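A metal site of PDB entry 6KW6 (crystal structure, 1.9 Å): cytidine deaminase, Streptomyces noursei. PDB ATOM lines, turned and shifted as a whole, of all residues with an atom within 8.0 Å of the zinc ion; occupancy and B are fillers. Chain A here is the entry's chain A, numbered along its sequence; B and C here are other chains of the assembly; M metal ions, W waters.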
ATOM      1  N   VAL A  34      24.201  29.716 -19.005  1.00  0.00           N
ATOM      2  CA  VAL A  34      23.996  29.154 -17.675  1.00  0.00           C
ATOM      3  C   VAL A  34      24.816  27.874 -17.557  1.00  0.00           C
ATOM      4  O   VAL A  34      24.889  27.086 -18.509  1.00  0.00           O
ATOM      5  CB  VAL A  34      22.500  28.853 -17.394  1.00  0.00           C
ATOM      6  CG1 VAL A  34      22.333  28.273 -15.992  1.00  0.00           C
ATOM      7  CG2 VAL A  34      21.649  30.104 -17.545  1.00  0.00           C
ATOM      8  N   ASN A  50      23.334  25.311 -20.657  1.00  0.00           N
ATOM      9  CA  ASN A  50      22.110  25.387 -21.428  1.00  0.00           C
ATOM     10  C   ASN A  50      22.427  25.389 -22.910  1.00  0.00           C
ATOM     11  O   ASN A  50      23.527  25.746 -23.343  1.00  0.00           O
ATOM     12  CB  ASN A  50      21.243  26.596 -21.036  1.00  0.00           C
ATOM     13  CG  ASN A  50      21.926  27.941 -21.184  1.00  0.00           C
ATOM     14  OD1 ASN A  50      23.159  28.048 -21.147  1.00  0.00           O
ATOM     15  ND2 ASN A  50      21.124  28.996 -21.309  1.00  0.00           N
ATOM     16  N   GLY A  59      14.549  24.622 -26.135  1.00  0.00           N
ATOM     17  CA  GLY A  59      15.801  24.846 -25.427  1.00  0.00           C
ATOM     18  C   GLY A  59      15.948  23.902 -24.244  1.00  0.00           C
ATOM     19  O   GLY A  59      14.975  23.506 -23.610  1.00  0.00           O
ATOM     20  N   LEU A  60      17.198  23.527 -23.978  1.00  0.00           N
ATOM     21  CA  LEU A  60      17.524  22.672 -22.849  1.00  0.00           C
ATOM     22  C   LEU A  60      18.198  23.506 -21.766  1.00  0.00           C
ATOM     23  O   LEU A  60      19.139  24.252 -22.059  1.00  0.00           O
ATOM     24  CB  LEU A  60      18.433  21.524 -23.288  1.00  0.00           C
ATOM     25  CG  LEU A  60      17.813  20.631 -24.364  1.00  0.00           C
ATOM     26  CD1 LEU A  60      18.866  19.858 -25.167  1.00  0.00           C
ATOM     27  CD2 LEU A  60      16.810  19.687 -23.707  1.00  0.00           C
ATOM     28  N   CYS A  61      17.683  23.428 -20.528  1.00  0.00           N
ATOM     29  CA  CYS A  61      18.346  24.137 -19.439  1.00  0.00           C
ATOM     30  C   CYS A  61      19.655  23.438 -19.081  1.00  0.00           C
ATOM     31  O   CYS A  61      19.885  22.279 -19.449  1.00  0.00           O
ATOM     32  CB  CYS A  61      17.434  24.196 -18.195  1.00  0.00           C
ATOM     33  SG  CYS A  61      15.928  25.263 -18.283  1.00  0.00           S
ATOM     34  N   ALA A  62      20.526  24.152 -18.359  1.00  0.00           N
ATOM     35  CA  ALA A  62      21.754  23.519 -17.884  1.00  0.00           C
ATOM     36  C   ALA A  62      21.442  22.300 -17.026  1.00  0.00           C
ATOM     37  O   ALA A  62      22.177  21.303 -17.071  1.00  0.00           O
ATOM     38  CB  ALA A  62      22.596  24.513 -17.073  1.00  0.00           C
ATOM     39  N   GLU A  63      20.371  22.349 -16.248  1.00  0.00           N
ATOM     40  CA  GLU A  63      20.053  21.204 -15.404  1.00  0.00           C
ATOM     41  C   GLU A  63      19.596  20.008 -16.238  1.00  0.00           C
ATOM     42  O   GLU A  63      19.852  18.863 -15.853  1.00  0.00           O
ATOM     43  CB  GLU A  63      18.986  21.592 -14.368  1.00  0.00           C
ATOM     44  CG  GLU A  63      19.399  22.781 -13.488  1.00  0.00           C
ATOM     45  CD  GLU A  63      18.983  24.145 -14.047  1.00  0.00           C
ATOM     46  OE1 GLU A  63      19.229  24.422 -15.240  1.00  0.00           O
ATOM     47  OE2 GLU A  63      18.417  24.957 -13.293  1.00  0.00           O
ATOM     48  N   CYS A  64      18.971  20.243 -17.400  1.00  0.00           N
ATOM     49  CA  CYS A  64      18.674  19.146 -18.319  1.00  0.00           C
ATOM     50  C   CYS A  64      19.944  18.430 -18.743  1.00  0.00           C
ATOM     51  O   CYS A  64      20.048  17.193 -18.654  1.00  0.00           O
ATOM     52  CB  CYS A  64      17.931  19.653 -19.557  1.00  0.00           C
ATOM     53  SG  CYS A  64      16.357  20.443 -19.214  1.00  0.00           S
ATOM     54  N   CYS A  83      24.133  26.273  -9.575  1.00  0.00           N
ATOM     55  CA  CYS A  83      23.828  26.829 -10.890  1.00  0.00           C
ATOM     56  C   CYS A  83      24.275  28.280 -10.927  1.00  0.00           C
ATOM     57  O   CYS A  83      24.069  29.018  -9.963  1.00  0.00           O
ATOM     58  CB  CYS A  83      22.319  26.727 -11.171  1.00  0.00           C
ATOM     59  SG  CYS A  83      21.883  27.194 -12.826  1.00  0.00           S
ATOM     60  N   VAL A  92      18.649  30.129  -8.947  1.00  0.00           N
ATOM     61  CA  VAL A  92      17.751  29.068  -8.501  1.00  0.00           C
ATOM     62  C   VAL A  92      17.128  28.421  -9.729  1.00  0.00           C
ATOM     63  O   VAL A  92      16.599  29.136 -10.597  1.00  0.00           O
ATOM     64  CB  VAL A  92      16.678  29.594  -7.533  1.00  0.00           C
ATOM     65  CG1 VAL A  92      15.824  28.446  -7.022  1.00  0.00           C
ATOM     66  CG2 VAL A  92      17.326  30.318  -6.353  1.00  0.00           C
ATOM     67  N   PRO A  93      17.199  27.100  -9.866  1.00  0.00           N
ATOM     68  CA  PRO A  93      16.591  26.431 -11.030  1.00  0.00           C
ATOM     69  C   PRO A  93      15.139  26.830 -11.212  1.00  0.00           C
ATOM     70  O   PRO A  93      14.423  27.104 -10.244  1.00  0.00           O
ATOM     71  CB  PRO A  93      16.709  24.947 -10.677  1.00  0.00           C
ATOM     72  CG  PRO A  93      17.825  24.856  -9.709  1.00  0.00           C
ATOM     73  CD  PRO A  93      17.861  26.156  -8.953  1.00  0.00           C
ATOM     74  N   CYS A  94      14.696  26.861 -12.471  1.00  0.00           N
ATOM     75  CA  CYS A  94      13.281  27.032 -12.743  1.00  0.00           C
ATOM     76  C   CYS A  94      12.502  25.825 -12.236  1.00  0.00           C
ATOM     77  O   CYS A  94      13.084  24.796 -11.852  1.00  0.00           O
ATOM     78  CB  CYS A  94      13.047  27.250 -14.242  1.00  0.00           C
ATOM     79  SG  CYS A  94      13.046  25.760 -15.301  1.00  0.00           S
ATOM     80  N   GLY A  95      11.177  25.941 -12.239  1.00  0.00           N
ATOM     81  CA  GLY A  95      10.338  24.863 -11.733  1.00  0.00           C
ATOM     82  C   GLY A  95      10.551  23.551 -12.457  1.00  0.00           C
ATOM     83  O   GLY A  95      10.583  22.481 -11.843  1.00  0.00           O
ATOM     84  N   ARG A  96      10.709  23.608 -13.793  1.00  0.00           N
ATOM     85  CA  ARG A  96      10.950  22.377 -14.546  1.00  0.00           C
ATOM     86  C   ARG A  96      12.203  21.663 -14.058  1.00  0.00           C
ATOM     87  O   ARG A  96      12.189  20.446 -13.820  1.00  0.00           O
ATOM     88  CB  ARG A  96      11.080  22.700 -16.036  1.00  0.00           C
ATOM     89  CG  ARG A  96      11.261  21.452 -16.904  1.00  0.00           C
ATOM     90  CD  ARG A  96      12.727  21.176 -17.199  1.00  0.00           C
ATOM     91  NE  ARG A  96      13.352  22.256 -17.963  1.00  0.00           N
ATOM     92  CZ  ARG A  96      13.292  22.358 -19.290  1.00  0.00           C
ATOM     93  NH1 ARG A  96      12.623  21.460 -19.992  1.00  0.00           N
ATOM     94  NH2 ARG A  96      13.897  23.371 -19.906  1.00  0.00           N
ATOM     95  N   CYS A  97      13.297  22.405 -13.913  1.00  0.00           N
ATOM     96  CA  CYS A  97      14.547  21.839 -13.444  1.00  0.00           C
ATOM     97  C   CYS A  97      14.483  21.401 -11.978  1.00  0.00           C
ATOM     98  O   CYS A  97      15.122  20.415 -11.606  1.00  0.00           O
ATOM     99  CB  CYS A  97      15.662  22.842 -13.682  1.00  0.00           C
ATOM    100  SG  CYS A  97      15.934  23.069 -15.472  1.00  0.00           S
ATOM    101  N   ARG A  98      13.700  22.101 -11.141  1.00  0.00           N
ATOM    102  CA  ARG A  98      13.464  21.600  -9.780  1.00  0.00           C
ATOM    103  C   ARG A  98      12.847  20.212  -9.814  1.00  0.00           C
ATOM    104  O   ARG A  98      13.190  19.358  -8.984  1.00  0.00           O
ATOM    105  CB  ARG A  98      12.553  22.543  -9.013  1.00  0.00           C
ATOM    106  CG  ARG A  98      13.182  23.865  -8.732  1.00  0.00           C
ATOM    107  CD  ARG A  98      12.269  24.773  -7.937  1.00  0.00           C
ATOM    108  NE  ARG A  98      12.648  26.158  -8.169  1.00  0.00           N
ATOM    109  CZ  ARG A  98      12.220  27.185  -7.450  1.00  0.00           C
ATOM    110  NH1 ARG A  98      11.400  27.001  -6.421  1.00  0.00           N
ATOM    111  NH2 ARG A  98      12.627  28.412  -7.765  1.00  0.00           N
ATOM    112  N   LEU A 100      13.160  17.948 -12.299  1.00  0.00           N
ATOM    113  CA  LEU A 100      14.211  17.026 -12.724  1.00  0.00           C
ATOM    114  C   LEU A 100      15.138  16.686 -11.567  1.00  0.00           C
ATOM    115  O   LEU A 100      15.512  15.522 -11.372  1.00  0.00           O
ATOM    116  CB  LEU A 100      15.029  17.640 -13.861  1.00  0.00           C
ATOM    117  CG  LEU A 100      14.330  17.913 -15.198  1.00  0.00           C
ATOM    118  CD1 LEU A 100      15.331  18.499 -16.191  1.00  0.00           C
ATOM    119  CD2 LEU A 100      13.687  16.655 -15.737  1.00  0.00           C
ATOM    120  N   SER B  55      11.531  31.207 -18.480  1.00  0.00           N
ATOM    121  CA  SER B  55      12.393  30.069 -18.804  1.00  0.00           C
ATOM    122  C   SER B  55      12.041  29.633 -20.221  1.00  0.00           C
ATOM    123  O   SER B  55      11.013  28.993 -20.433  1.00  0.00           O
ATOM    124  CB  SER B  55      12.209  28.937 -17.800  1.00  0.00           C
ATOM    125  OG  SER B  55      12.940  27.790 -18.172  1.00  0.00           O
ATOM    126  N   TYR B  56      12.911  29.990 -21.177  1.00  0.00           N
ATOM    127  CA  TYR B  56      12.567  29.853 -22.595  1.00  0.00           C
ATOM    128  C   TYR B  56      12.111  28.456 -22.947  1.00  0.00           C
ATOM    129  O   TYR B  56      11.148  28.272 -23.708  1.00  0.00           O
ATOM    130  CB  TYR B  56      13.772  30.198 -23.485  1.00  0.00           C
ATOM    131  CG  TYR B  56      14.092  31.655 -23.634  1.00  0.00           C
ATOM    132  CD1 TYR B  56      13.730  32.586 -22.676  1.00  0.00           C
ATOM    133  CD2 TYR B  56      14.772  32.112 -24.768  1.00  0.00           C
ATOM    134  CE1 TYR B  56      14.029  33.922 -22.820  1.00  0.00           C
ATOM    135  CE2 TYR B  56      15.066  33.435 -24.929  1.00  0.00           C
ATOM    136  CZ  TYR B  56      14.705  34.336 -23.955  1.00  0.00           C
ATOM    137  OH  TYR B  56      15.014  35.672 -24.130  1.00  0.00           O
ATOM    138  N   GLY B  57      12.795  27.438 -22.410  1.00  0.00           N
ATOM    139  CA  GLY B  57      12.504  26.057 -22.729  1.00  0.00           C
ATOM    140  C   GLY B  57      11.146  25.596 -22.283  1.00  0.00           C
ATOM    141  O   GLY B  57      10.736  24.483 -22.647  1.00  0.00           O
ATOM    142  N   LEU B  58      10.441  26.399 -21.495  1.00  0.00           N
ATOM    143  CA  LEU B  58       9.086  26.071 -21.077  1.00  0.00           C
ATOM    144  C   LEU B  58       8.036  26.717 -21.979  1.00  0.00           C
ATOM    145  O   LEU B  58       6.838  26.546 -21.729  1.00  0.00           O
ATOM    146  CB  LEU B  58       8.854  26.498 -19.629  1.00  0.00           C
ATOM    147  CG  LEU B  58       9.850  25.878 -18.646  1.00  0.00           C
ATOM    148  CD1 LEU B  58       9.399  26.129 -17.204  1.00  0.00           C
ATOM    149  CD2 LEU B  58       9.999  24.387 -18.929  1.00  0.00           C
ATOM    150  N   GLN C  99       5.943  26.549 -12.652  1.00  0.00           N
ATOM    151  CA  GLN C  99       6.629  27.675 -13.267  1.00  0.00           C
ATOM    152  C   GLN C  99       5.711  28.372 -14.272  1.00  0.00           C
ATOM    153  O   GLN C  99       5.731  29.599 -14.360  1.00  0.00           O
ATOM    154  CB  GLN C  99       7.919  27.214 -13.919  1.00  0.00           C
ATOM    155  CG  GLN C  99       8.822  28.379 -14.376  1.00  0.00           C
ATOM    156  CD  GLN C  99       9.451  29.109 -13.196  1.00  0.00           C
ATOM    157  OE1 GLN C  99      10.167  28.510 -12.398  1.00  0.00           O
ATOM    158  NE2 GLN C  99       9.172  30.411 -13.078  1.00  0.00           N
HETATM  159 ZN    ZN M   1      15.296  25.198 -15.953  1.00  0.00          ZN
HETATM  160  O   HOH W   1      16.587  26.370 -14.694  1.00  0.00           O
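The side-chain sulfur (SG) of Cys 61 sits close to the guanidinium group (NH2) of Arg 96 (3.2 Å).
The side-chain sulfur (SG) of Cys 94 lies close to the backbone NH (N) of Arg 96 (3.5 Å).
The side-chain sulfur (SG) of Cys 94 lies close to the side-chain hydroxyl (OG) of Ser 55 of chain B (3.5 Å).
SG of Cys 97 lies close to OE1 of Glu 63 (3.6 Å).
The backbone NH (N) of Cys 61 is in hydrogen-bond range of the side-chain sulfur (SG) of Cys 64 (3.5 Å).
The side-chain sulfur (SG) of Cys 97 sits close to the guanidinium group (NE) of Arg 96 (3.7 Å).
Water W1 lies within hydrogen-bond range of OE2 of Glu 63 (2.7 Å) and N of Cys 94 (3.0 Å).
The zinc ion is bound by water W1 (2.2 Å), SG of Cys 97 (2.3 Å), SG of Cys 94 (2.4 Å) and SG of Cys 61 (2.4 Å).
Three residues have an atom within 4 Å of the zinc ion: Cys 61, Cys 94 and Cys 97.
The nearest printed residue that does not touch the zinc ion is Arg 96 (4.1 Å).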
